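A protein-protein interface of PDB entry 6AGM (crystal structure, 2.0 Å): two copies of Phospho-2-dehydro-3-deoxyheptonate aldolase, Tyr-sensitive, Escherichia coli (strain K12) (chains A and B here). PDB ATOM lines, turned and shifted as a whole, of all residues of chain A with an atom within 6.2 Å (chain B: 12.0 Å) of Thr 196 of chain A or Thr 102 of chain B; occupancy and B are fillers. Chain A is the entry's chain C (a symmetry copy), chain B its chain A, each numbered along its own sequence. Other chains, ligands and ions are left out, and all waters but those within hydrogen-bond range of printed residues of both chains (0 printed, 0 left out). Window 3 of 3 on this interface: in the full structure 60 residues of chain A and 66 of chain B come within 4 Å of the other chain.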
ATOM      1  N   THR A 168     -17.754  11.471 -30.174  1.00  0.00           N
ATOM      2  CA  THR A 168     -16.501  12.212 -30.095  1.00  0.00           C
ATOM      3  C   THR A 168     -16.580  13.423 -29.172  1.00  0.00           C
ATOM      4  O   THR A 168     -15.535  13.903 -28.719  1.00  0.00           O
ATOM      5  CB  THR A 168     -16.065  12.662 -31.492  1.00  0.00           C
ATOM      6  OG1 THR A 168     -17.016  13.596 -32.015  1.00  0.00           O
ATOM      7  CG2 THR A 168     -15.972  11.465 -32.431  1.00  0.00           C
ATOM      8  N   GLU A 169     -17.777  13.930 -28.880  1.00  0.00           N
ATOM      9  CA  GLU A 169     -17.913  15.086 -28.003  1.00  0.00           C
ATOM     10  C   GLU A 169     -18.254  14.709 -26.568  1.00  0.00           C
ATOM     11  O   GLU A 169     -18.362  15.596 -25.716  1.00  0.00           O
ATOM     12  CB  GLU A 169     -18.960  16.057 -28.558  1.00  0.00           C
ATOM     13  CG  GLU A 169     -18.497  16.766 -29.822  1.00  0.00           C
ATOM     14  CD  GLU A 169     -19.434  17.875 -30.256  1.00  0.00           C
ATOM     15  OE1 GLU A 169     -20.526  18.001 -29.664  1.00  0.00           O
ATOM     16  OE2 GLU A 169     -19.077  18.619 -31.192  1.00  0.00           O
ATOM     17  N   GLN A 171     -16.771  12.829 -23.105  1.00  0.00           N
ATOM     18  CA  GLN A 171     -15.459  12.554 -22.535  1.00  0.00           C
ATOM     19  C   GLN A 171     -15.353  11.156 -21.954  1.00  0.00           C
ATOM     20  O   GLN A 171     -14.256  10.594 -21.927  1.00  0.00           O
ATOM     21  CB  GLN A 171     -15.115  13.573 -21.443  1.00  0.00           C
ATOM     22  CG  GLN A 171     -13.642  13.925 -21.351  1.00  0.00           C
ATOM     23  CD  GLN A 171     -13.248  15.062 -22.271  1.00  0.00           C
ATOM     24  OE1 GLN A 171     -12.747  14.837 -23.367  1.00  0.00           O
ATOM     25  NE2 GLN A 171     -13.475  16.294 -21.824  1.00  0.00           N
ATOM     26  N   ARG A 174     -15.222   9.075 -25.697  1.00  0.00           N
ATOM     27  CA  ARG A 174     -14.838   9.701 -26.962  1.00  0.00           C
ATOM     28  C   ARG A 174     -13.973   8.777 -27.817  1.00  0.00           C
ATOM     29  O   ARG A 174     -13.957   8.900 -29.047  1.00  0.00           O
ATOM     30  CB  ARG A 174     -14.119  11.024 -26.686  1.00  0.00           C
ATOM     31  CG  ARG A 174     -13.034  11.416 -27.677  1.00  0.00           C
ATOM     32  CD  ARG A 174     -12.141  12.514 -27.127  1.00  0.00           C
ATOM     33  NE  ARG A 174     -12.901  13.720 -26.809  1.00  0.00           N
ATOM     34  CZ  ARG A 174     -12.369  14.823 -26.293  1.00  0.00           C
ATOM     35  NH1 ARG A 174     -11.070  14.872 -26.029  1.00  0.00           N
ATOM     36  NH2 ARG A 174     -13.138  15.872 -26.026  1.00  0.00           N
ATOM     37  N   GLU A 175     -13.263   7.836 -27.190  1.00  0.00           N
ATOM     38  CA  GLU A 175     -12.376   6.920 -27.895  1.00  0.00           C
ATOM     39  C   GLU A 175     -13.009   5.556 -28.138  1.00  0.00           C
ATOM     40  O   GLU A 175     -12.285   4.573 -28.325  1.00  0.00           O
ATOM     41  CB  GLU A 175     -11.069   6.757 -27.118  1.00  0.00           C
ATOM     42  CG  GLU A 175     -10.505   8.045 -26.541  1.00  0.00           C
ATOM     43  CD  GLU A 175     -10.000   8.997 -27.610  1.00  0.00           C
ATOM     44  OE1 GLU A 175      -9.667  10.152 -27.271  1.00  0.00           O
ATOM     45  OE2 GLU A 175      -9.935   8.592 -28.793  1.00  0.00           O
ATOM     46  N   PHE A 186     -16.115   8.298 -39.920  1.00  0.00           N
ATOM     47  CA  PHE A 186     -16.176   9.436 -39.007  1.00  0.00           C
ATOM     48  C   PHE A 186     -16.789  10.638 -39.712  1.00  0.00           C
ATOM     49  O   PHE A 186     -16.218  11.151 -40.681  1.00  0.00           O
ATOM     50  CB  PHE A 186     -14.781   9.762 -38.477  1.00  0.00           C
ATOM     51  CG  PHE A 186     -14.187   8.655 -37.668  1.00  0.00           C
ATOM     52  CD1 PHE A 186     -13.421   7.671 -38.273  1.00  0.00           C
ATOM     53  CD2 PHE A 186     -14.426   8.574 -36.307  1.00  0.00           C
ATOM     54  CE1 PHE A 186     -12.889   6.633 -37.529  1.00  0.00           C
ATOM     55  CE2 PHE A 186     -13.895   7.541 -35.556  1.00  0.00           C
ATOM     56  CZ  PHE A 186     -13.130   6.570 -36.170  1.00  0.00           C
ATOM     57  N   LYS A 187     -17.939  11.093 -39.213  1.00  0.00           N
ATOM     58  CA  LYS A 187     -18.635  12.210 -39.842  1.00  0.00           C
ATOM     59  C   LYS A 187     -17.919  13.527 -39.564  1.00  0.00           C
ATOM     60  O   LYS A 187     -17.349  13.728 -38.488  1.00  0.00           O
ATOM     61  CB  LYS A 187     -20.079  12.285 -39.342  1.00  0.00           C
ATOM     62  CG  LYS A 187     -20.925  11.070 -39.698  1.00  0.00           C
ATOM     63  CD  LYS A 187     -22.022  10.822 -38.669  1.00  0.00           C
ATOM     64  CE  LYS A 187     -23.271  11.627 -38.975  1.00  0.00           C
ATOM     65  NZ  LYS A 187     -24.344  11.402 -37.962  1.00  0.00           N
ATOM     66  N   ASN A 188     -17.945  14.428 -40.545  1.00  0.00           N
ATOM     67  CA  ASN A 188     -17.384  15.754 -40.341  1.00  0.00           C
ATOM     68  C   ASN A 188     -18.270  16.560 -39.392  1.00  0.00           C
ATOM     69  O   ASN A 188     -19.420  16.203 -39.114  1.00  0.00           O
ATOM     70  CB  ASN A 188     -17.208  16.485 -41.675  1.00  0.00           C
ATOM     71  CG  ASN A 188     -18.528  16.743 -42.393  1.00  0.00           C
ATOM     72  OD1 ASN A 188     -18.898  16.018 -43.317  1.00  0.00           O
ATOM     73  ND2 ASN A 188     -19.232  17.793 -41.982  1.00  0.00           N
ATOM     74  N   GLY A 189     -17.718  17.663 -38.890  1.00  0.00           N
ATOM     75  CA  GLY A 189     -18.451  18.495 -37.955  1.00  0.00           C
ATOM     76  C   GLY A 189     -19.708  19.084 -38.564  1.00  0.00           C
ATOM     77  O   GLY A 189     -19.851  19.202 -39.783  1.00  0.00           O
ATOM     78  N   THR A 190     -20.643  19.455 -37.683  1.00  0.00           N
ATOM     79  CA  THR A 190     -21.902  20.039 -38.138  1.00  0.00           C
ATOM     80  C   THR A 190     -21.680  21.365 -38.854  1.00  0.00           C
ATOM     81  O   THR A 190     -22.433  21.709 -39.773  1.00  0.00           O
ATOM     82  CB  THR A 190     -22.853  20.237 -36.956  1.00  0.00           C
ATOM     83  OG1 THR A 190     -22.669  19.177 -36.009  1.00  0.00           O
ATOM     84  CG2 THR A 190     -24.298  20.238 -37.432  1.00  0.00           C
ATOM     85  N   ASP A 191     -20.659  22.118 -38.451  1.00  0.00           N
ATOM     86  CA  ASP A 191     -20.308  23.360 -39.127  1.00  0.00           C
ATOM     87  C   ASP A 191     -19.574  23.127 -40.439  1.00  0.00           C
ATOM     88  O   ASP A 191     -19.352  24.087 -41.185  1.00  0.00           O
ATOM     89  CB  ASP A 191     -19.441  24.227 -38.211  1.00  0.00           C
ATOM     90  CG  ASP A 191     -18.208  23.493 -37.714  1.00  0.00           C
ATOM     91  OD1 ASP A 191     -18.295  22.267 -37.490  1.00  0.00           O
ATOM     92  OD2 ASP A 191     -17.150  24.140 -37.553  1.00  0.00           O
ATOM     93  N   SER A 193     -16.531  21.343 -40.323  1.00  0.00           N
ATOM     94  CA  SER A 193     -15.133  21.158 -39.961  1.00  0.00           C
ATOM     95  C   SER A 193     -14.697  19.729 -40.258  1.00  0.00           C
ATOM     96  O   SER A 193     -15.302  18.769 -39.769  1.00  0.00           O
ATOM     97  CB  SER A 193     -14.921  21.483 -38.485  1.00  0.00           C
ATOM     98  OG  SER A 193     -13.637  21.064 -38.054  1.00  0.00           O
ATOM     99  N   LEU A 194     -13.649  19.590 -41.066  1.00  0.00           N
ATOM    100  CA  LEU A 194     -13.051  18.285 -41.299  1.00  0.00           C
ATOM    101  C   LEU A 194     -12.100  17.886 -40.181  1.00  0.00           C
ATOM    102  O   LEU A 194     -11.782  16.698 -40.048  1.00  0.00           O
ATOM    103  CB  LEU A 194     -12.314  18.289 -42.639  1.00  0.00           C
ATOM    104  CG  LEU A 194     -13.204  18.672 -43.823  1.00  0.00           C
ATOM    105  CD1 LEU A 194     -12.416  18.656 -45.115  1.00  0.00           C
ATOM    106  CD2 LEU A 194     -14.404  17.739 -43.909  1.00  0.00           C
ATOM    107  N   ALA A 195     -11.659  18.855 -39.375  1.00  0.00           N
ATOM    108  CA  ALA A 195     -10.661  18.586 -38.345  1.00  0.00           C
ATOM    109  C   ALA A 195     -11.162  17.569 -37.329  1.00  0.00           C
ATOM    110  O   ALA A 195     -10.413  16.680 -36.916  1.00  0.00           O
ATOM    111  CB  ALA A 195     -10.266  19.889 -37.649  1.00  0.00           C
ATOM    112  N   THR A 196     -12.420  17.691 -36.901  1.00  0.00           N
ATOM    113  CA  THR A 196     -12.951  16.761 -35.909  1.00  0.00           C
ATOM    114  C   THR A 196     -12.915  15.328 -36.430  1.00  0.00           C
ATOM    115  O   THR A 196     -12.431  14.417 -35.747  1.00  0.00           O
ATOM    116  CB  THR A 196     -14.372  17.161 -35.520  1.00  0.00           C
ATOM    117  OG1 THR A 196     -15.185  17.248 -36.696  1.00  0.00           O
ATOM    118  CG2 THR A 196     -14.366  18.506 -34.814  1.00  0.00           C
ATOM    119  N   ALA A 197     -13.404  15.119 -37.655  1.00  0.00           N
ATOM    120  CA  ALA A 197     -13.411  13.779 -38.234  1.00  0.00           C
ATOM    121  C   ALA A 197     -11.996  13.251 -38.435  1.00  0.00           C
ATOM    122  O   ALA A 197     -11.725  12.074 -38.174  1.00  0.00           O
ATOM    123  CB  ALA A 197     -14.171  13.785 -39.560  1.00  0.00           C
ATOM    124  N   ILE A 198     -11.080  14.105 -38.896  1.00  0.00           N
ATOM    125  CA  ILE A 198      -9.714  13.660 -39.159  1.00  0.00           C
ATOM    126  C   ILE A 198      -9.017  13.268 -37.859  1.00  0.00           C
ATOM    127  O   ILE A 198      -8.359  12.222 -37.778  1.00  0.00           O
ATOM    128  CB  ILE A 198      -8.935  14.748 -39.917  1.00  0.00           C
ATOM    129  CG1 ILE A 198      -9.489  14.898 -41.334  1.00  0.00           C
ATOM    130  CG2 ILE A 198      -7.453  14.419 -39.959  1.00  0.00           C
ATOM    131  CD1 ILE A 198      -8.911  16.074 -42.088  1.00  0.00           C
ATOM    132  N   ASN A 199      -9.152  14.102 -36.825  1.00  0.00           N
ATOM    133  CA  ASN A 199      -8.563  13.780 -35.530  1.00  0.00           C
ATOM    134  C   ASN A 199      -9.169  12.510 -34.949  1.00  0.00           C
ATOM    135  O   ASN A 199      -8.449  11.674 -34.392  1.00  0.00           O
ATOM    136  CB  ASN A 199      -8.743  14.950 -34.561  1.00  0.00           C
ATOM    137  CG  ASN A 199      -8.078  16.224 -35.048  1.00  0.00           C
ATOM    138  OD1 ASN A 199      -7.074  16.183 -35.759  1.00  0.00           O
ATOM    139  ND2 ASN A 199      -8.636  17.367 -34.664  1.00  0.00           N
ATOM    140  N   ALA A 200     -10.490  12.342 -35.071  1.00  0.00           N
ATOM    141  CA  ALA A 200     -11.132  11.140 -34.548  1.00  0.00           C
ATOM    142  C   ALA A 200     -10.660   9.895 -35.289  1.00  0.00           C
ATOM    143  O   ALA A 200     -10.404   8.856 -34.672  1.00  0.00           O
ATOM    144  CB  ALA A 200     -12.651  11.276 -34.641  1.00  0.00           C
ATOM    145  N   MET A 201     -10.535   9.985 -36.615  1.00  0.00           N
ATOM    146  CA  MET A 201     -10.066   8.852 -37.402  1.00  0.00           C
ATOM    147  C   MET A 201      -8.636   8.481 -37.037  1.00  0.00           C
ATOM    148  O   MET A 201      -8.315   7.297 -36.880  1.00  0.00           O
ATOM    149  CB  MET A 201     -10.178   9.176 -38.893  1.00  0.00           C
ATOM    150  CG  MET A 201      -9.514   8.160 -39.811  1.00  0.00           C
ATOM    151  SD  MET A 201      -9.713   8.608 -41.547  1.00  0.00           S
ATOM    152  CE  MET A 201      -8.573   7.470 -42.329  1.00  0.00           C
ATOM    153  N   GLU B  97     -15.938  18.455 -16.569  1.00  0.00           N
ATOM    154  CA  GLU B  97     -15.840  18.137 -17.980  1.00  0.00           C
ATOM    155  C   GLU B  97     -16.187  19.362 -18.810  1.00  0.00           C
ATOM    156  O   GLU B  97     -17.086  20.133 -18.461  1.00  0.00           O
ATOM    157  CB  GLU B  97     -16.786  16.983 -18.315  1.00  0.00           C
ATOM    158  CG  GLU B  97     -16.663  16.405 -19.710  1.00  0.00           C
ATOM    159  CD  GLU B  97     -17.891  15.590 -20.080  1.00  0.00           C
ATOM    160  OE1 GLU B  97     -18.934  15.769 -19.417  1.00  0.00           O
ATOM    161  OE2 GLU B  97     -17.825  14.778 -21.025  1.00  0.00           O
ATOM    162  N   LYS B  98     -15.454  19.547 -19.892  1.00  0.00           N
ATOM    163  CA  LYS B  98     -16.108  20.515 -20.756  1.00  0.00           C
ATOM    164  C   LYS B  98     -16.995  19.785 -21.756  1.00  0.00           C
ATOM    165  O   LYS B  98     -16.649  18.689 -22.203  1.00  0.00           O
ATOM    166  CB  LYS B  98     -15.082  21.349 -21.518  1.00  0.00           C
ATOM    167  CG  LYS B  98     -14.975  22.802 -21.096  1.00  0.00           C
ATOM    168  CD  LYS B  98     -13.934  23.524 -21.944  1.00  0.00           C
ATOM    169  CE  LYS B  98     -13.693  24.948 -21.466  1.00  0.00           C
ATOM    170  NZ  LYS B  98     -13.227  24.987 -20.054  1.00  0.00           N
ATOM    171  N   PRO B  99     -18.146  20.344 -22.124  1.00  0.00           N
ATOM    172  CA  PRO B  99     -18.747  19.958 -23.405  1.00  0.00           C
ATOM    173  C   PRO B  99     -17.879  20.529 -24.519  1.00  0.00           C
ATOM    174  O   PRO B  99     -16.830  21.109 -24.226  1.00  0.00           O
ATOM    175  CB  PRO B  99     -20.146  20.595 -23.363  1.00  0.00           C
ATOM    176  CG  PRO B  99     -20.332  21.092 -21.948  1.00  0.00           C
ATOM    177  CD  PRO B  99     -18.961  21.335 -21.404  1.00  0.00           C
ATOM    178  N   ARG B 100     -18.268  20.376 -25.784  1.00  0.00           N
ATOM    179  CA  ARG B 100     -17.674  21.150 -26.877  1.00  0.00           C
ATOM    180  C   ARG B 100     -16.155  20.938 -26.977  1.00  0.00           C
ATOM    181  O   ARG B 100     -15.365  21.846 -26.718  1.00  0.00           O
ATOM    182  CB  ARG B 100     -17.977  22.646 -26.692  1.00  0.00           C
ATOM    183  CG  ARG B 100     -19.289  23.016 -25.985  1.00  0.00           C
ATOM    184  CD  ARG B 100     -19.450  24.537 -25.949  1.00  0.00           C
ATOM    185  NE  ARG B 100     -20.684  24.958 -25.296  1.00  0.00           N
ATOM    186  CZ  ARG B 100     -20.782  25.339 -24.023  1.00  0.00           C
ATOM    187  NH1 ARG B 100     -19.722  25.337 -23.212  1.00  0.00           N
ATOM    188  NH2 ARG B 100     -21.967  25.702 -23.557  1.00  0.00           N
ATOM    189  N   THR B 101     -15.762  19.698 -27.302  1.00  0.00           N
ATOM    190  CA  THR B 101     -14.428  19.375 -27.830  1.00  0.00           C
ATOM    191  C   THR B 101     -14.311  17.922 -28.260  1.00  0.00           C
ATOM    192  O   THR B 101     -15.003  17.054 -27.722  1.00  0.00           O
ATOM    193  CB  THR B 101     -13.281  19.631 -26.836  1.00  0.00           C
ATOM    194  OG1 THR B 101     -13.681  19.317 -25.495  1.00  0.00           O
ATOM    195  CG2 THR B 101     -12.751  21.040 -26.959  1.00  0.00           C
ATOM    196  N   THR B 102     -13.427  17.650 -29.222  1.00  0.00           N
ATOM    197  CA  THR B 102     -13.029  16.287 -29.538  1.00  0.00           C
ATOM    198  C   THR B 102     -11.574  15.990 -29.200  1.00  0.00           C
ATOM    199  O   THR B 102     -11.156  14.832 -29.318  1.00  0.00           O
ATOM    200  CB  THR B 102     -13.276  15.970 -31.023  1.00  0.00           C
ATOM    201  OG1 THR B 102     -12.215  16.510 -31.821  1.00  0.00           O
ATOM    202  CG2 THR B 102     -14.606  16.550 -31.477  1.00  0.00           C
ATOM    203  N   VAL B 103     -10.792  16.994 -28.791  1.00  0.00           N
ATOM    204  CA  VAL B 103      -9.401  16.807 -28.398  1.00  0.00           C
ATOM    205  C   VAL B 103      -9.137  17.617 -27.135  1.00  0.00           C
ATOM    206  O   VAL B 103      -9.867  18.556 -26.808  1.00  0.00           O
ATOM    207  CB  VAL B 103      -8.413  17.228 -29.509  1.00  0.00           C
ATOM    208  CG1 VAL B 103      -8.473  16.256 -30.678  1.00  0.00           C
ATOM    209  CG2 VAL B 103      -8.713  18.647 -29.968  1.00  0.00           C
ATOM    210  N   GLY B 104      -8.080  17.243 -26.425  1.00  0.00           N
ATOM    211  CA  GLY B 104      -7.612  17.984 -25.271  1.00  0.00           C
ATOM    212  C   GLY B 104      -7.667  17.159 -24.001  1.00  0.00           C
ATOM    213  O   GLY B 104      -7.923  15.952 -24.013  1.00  0.00           O
ATOM    214  N   TRP B 105      -7.410  17.839 -22.886  1.00  0.00           N
ATOM    215  CA  TRP B 105      -7.478  17.216 -21.573  1.00  0.00           C
ATOM    216  C   TRP B 105      -8.906  16.787 -21.262  1.00  0.00           C
ATOM    217  O   TRP B 105      -9.864  17.506 -21.554  1.00  0.00           O
ATOM    218  CB  TRP B 105      -6.969  18.191 -20.512  1.00  0.00           C
ATOM    219  CG  TRP B 105      -6.958  17.660 -19.109  1.00  0.00           C
ATOM    220  CD1 TRP B 105      -6.414  16.486 -18.678  1.00  0.00           C
ATOM    221  CD2 TRP B 105      -7.497  18.303 -17.946  1.00  0.00           C
ATOM    222  NE1 TRP B 105      -6.589  16.353 -17.321  1.00  0.00           N
ATOM    223  CE2 TRP B 105      -7.251  17.456 -16.849  1.00  0.00           C
ATOM    224  CE3 TRP B 105      -8.170  19.511 -17.730  1.00  0.00           C
ATOM    225  CZ2 TRP B 105      -7.653  17.777 -15.553  1.00  0.00           C
ATOM    226  CZ3 TRP B 105      -8.568  19.827 -16.443  1.00  0.00           C
ATOM    227  CH2 TRP B 105      -8.309  18.963 -15.372  1.00  0.00           C
ATOM    228  N   LYS B 106      -9.045  15.608 -20.664  1.00  0.00           N
ATOM    229  CA  LYS B 106     -10.349  15.013 -20.408  1.00  0.00           C
ATOM    230  C   LYS B 106     -10.964  15.454 -19.086  1.00  0.00           C
ATOM    231  O   LYS B 106     -12.019  14.935 -18.706  1.00  0.00           O
ATOM    232  CB  LYS B 106     -10.244  13.487 -20.448  1.00  0.00           C
ATOM    233  CG  LYS B 106     -10.051  12.926 -21.845  1.00  0.00           C
ATOM    234  CD  LYS B 106      -9.560  11.495 -21.793  1.00  0.00           C
ATOM    235  CE  LYS B 106      -9.272  10.959 -23.183  1.00  0.00           C
ATOM    236  NZ  LYS B 106     -10.501  10.925 -24.021  1.00  0.00           N
ATOM    237  N   GLY B 107     -10.339  16.391 -18.380  1.00  0.00           N
ATOM    238  CA  GLY B 107     -10.885  16.900 -17.141  1.00  0.00           C
ATOM    239  C   GLY B 107     -10.438  16.109 -15.924  1.00  0.00           C
ATOM    240  O   GLY B 107      -9.842  15.033 -16.013  1.00  0.00           O
ATOM    241  N   ASN B 110     -11.814  12.257 -15.458  1.00  0.00           N
ATOM    242  CA  ASN B 110     -11.247  11.218 -16.308  1.00  0.00           C
ATOM    243  C   ASN B 110      -9.727  11.172 -16.206  1.00  0.00           C
ATOM    244  O   ASN B 110      -9.141  10.085 -16.181  1.00  0.00           O
ATOM    245  CB  ASN B 110     -11.687  11.435 -17.755  1.00  0.00           C
ATOM    246  CG  ASN B 110     -13.196  11.432 -17.905  1.00  0.00           C
ATOM    247  OD1 ASN B 110     -13.899  10.697 -17.213  1.00  0.00           O
ATOM    248  ND2 ASN B 110     -13.700  12.264 -18.800  1.00  0.00           N
ATOM    249  N   PHE B 118      -6.361   8.484 -18.185  1.00  0.00           N
ATOM    250  CA  PHE B 118      -7.749   8.010 -18.103  1.00  0.00           C
ATOM    251  C   PHE B 118      -7.967   7.131 -16.869  1.00  0.00           C
ATOM    252  O   PHE B 118      -8.410   5.985 -16.953  1.00  0.00           O
ATOM    253  CB  PHE B 118      -8.169   7.278 -19.385  1.00  0.00           C
ATOM    254  CG  PHE B 118      -9.642   7.383 -19.685  1.00  0.00           C
ATOM    255  CD1 PHE B 118     -10.500   6.332 -19.411  1.00  0.00           C
ATOM    256  CD2 PHE B 118     -10.167   8.539 -20.234  1.00  0.00           C
ATOM    257  CE1 PHE B 118     -11.855   6.433 -19.688  1.00  0.00           C
ATOM    258  CE2 PHE B 118     -11.520   8.648 -20.513  1.00  0.00           C
ATOM    259  CZ  PHE B 118     -12.365   7.595 -20.238  1.00  0.00           C
ATOM    260  N   ARG B 166     -26.947  17.395 -24.971  1.00  0.00           N
ATOM    261  CA  ARG B 166     -26.429  16.065 -24.655  1.00  0.00           C
ATOM    262  C   ARG B 166     -27.476  15.203 -23.961  1.00  0.00           C
ATOM    263  O   ARG B 166     -27.450  13.973 -24.086  1.00  0.00           O
ATOM    264  CB  ARG B 166     -25.175  16.182 -23.789  1.00  0.00           C
ATOM    265  CG  ARG B 166     -23.983  16.790 -24.512  1.00  0.00           C
ATOM    266  CD  ARG B 166     -22.697  16.075 -24.158  1.00  0.00           C
ATOM    267  NE  ARG B 166     -22.779  14.634 -24.384  1.00  0.00           N
ATOM    268  CZ  ARG B 166     -22.559  14.048 -25.558  1.00  0.00           C
ATOM    269  NH1 ARG B 166     -22.250  14.781 -26.620  1.00  0.00           N
ATOM    270  NH2 ARG B 166     -22.649  12.729 -25.671  1.00  0.00           N
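Thr 168 of chain A touches Thr 102 of chain B. Thr 101 of chain B touches Glu 169 of chain A. NH1 of Arg 166 of chain B touches C of Glu 169 of chain A, at 3.997 Å. O of Lys 98 of chain B touches NE2 of Gln 171 of chain A, at 3.99 Å. NE2 of Gln 171 of chain A touches O of Trp 105 of chain B, at 3.8 Å. Gln 171 of chain A touches Lys 106 of chain B (CG to O, 3.3 Å). Asn 110 of chain B touches Gln 171 of chain A. Gln 171 of chain A touches Phe 118 of chain B. Arg 174 of chain A touches Gly 104 of chain B. Lys 106 of chain B touches Arg 174 of chain A.
Thr 196 of chain A touches just one residue of chain B: Thr 102 (3.9 Å). Of chain A, only Thr 168 (3.6 Å), Arg 174 (3.2 Å) and Thr 196 (3.9 Å) come within 4 Å of Thr 102 of chain B. Arg 174 of chain A touches just these residues of chain B: Thr 101 (2.8 Å), Thr 102 (3.2 Å), Val 103 (3.5 Å), Gly 104 (3.8 Å) and Lys 106 (3.9 Å). No residue of chain B comes within 4 Å of Gly 189 of chain A. Ala 197 of chain A touches none of the printed residues of chain B. No residue of chain B comes within 4 Å of Asn 199 of chain A. No residue of chain B comes within 4 Å of Ala 200 of chain A. Printed residues of chain A within 4 Å of Phe 118 of chain B: Gln 171. Of the printed residues of chain A, Gly 104 of chain B touches Arg 174 (3.8 Å). Printed residues of chain A within 4 Å of Asn 110 of chain B: Gln 171. Pro 99 of chain B touches none of the printed residues of chain A. Asp 191 of chain A touches none of the printed residues of chain B.
Of the 20 printed residues of chain A, 6 touch a printed residue of chain B. Of the 14 printed residues of chain B, 11 touch a printed residue of chain A. Printed residues of chain B that touch a printed residue of chain A: Glu 97, Lys 98, Thr 101, Thr 102, Val 103, Gly 104, Trp 105, Lys 106, Asn 110, Phe 118 and Arg 166. Along chain B the printed residues that touch a printed residue of chain A span positions 97 to 166. Among the printed residues, 17 pairs touch across the chains.
No position is printed for both chains. Of the 17 pairs that touch across the chains among the printed residues, none has its exchanged pair printed and touching as well.
ND2 of Asn 110 of chain B is in hydrogen-bond range of O of Lys 106 of chain B (3.2 Å). O of Thr 168 of chain A is in hydrogen-bond range of NE of Arg 174 of chain A, 3.3 Å away. The guanidinium group (NH2) of Arg 174 of chain A is in hydrogen-bond range of the side-chain amide oxygen (OE1) of Gln 171 of chain A, at 2.9 Å. The side-chain hydroxyl of Thr 196 of chain A sits at hydrogen-bond distance from the backbone NH of Gly 189 of chain A. The backbone carbonyl oxygen (O) of Ser 193 of chain A is in hydrogen-bond range of the side-chain hydroxyl (OG1) of Thr 196 of chain A (3.4 Å).
The side-chain carboxylate (OE2) of Glu 97 of chain B sits close to the backbone NH (N) of Gln 171 of chain A, 3.0 Å away. The guanidinium group of Arg 174 of chain A sits at hydrogen-bond distance from the backbone carbonyl oxygen of Thr 101 of chain B (2.8 Å). The backbone carbonyl oxygen of Thr 102 of chain B lies within hydrogen-bond range of the guanidinium group of Arg 174 of chain A (3.3 Å). The side-chain carboxylate (OE1) of Glu 175 of chain A lies within salt-bridge range of the side-chain amino group (NZ) of Lys 106 of chain B, at 3.4 Å. O of Thr 168 of chain A lies close to O of Thr 101 of chain B, at 3.3 Å. The backbone NH of Val 103 of chain B sits close to the guanidinium group of Arg 174 of chain A.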
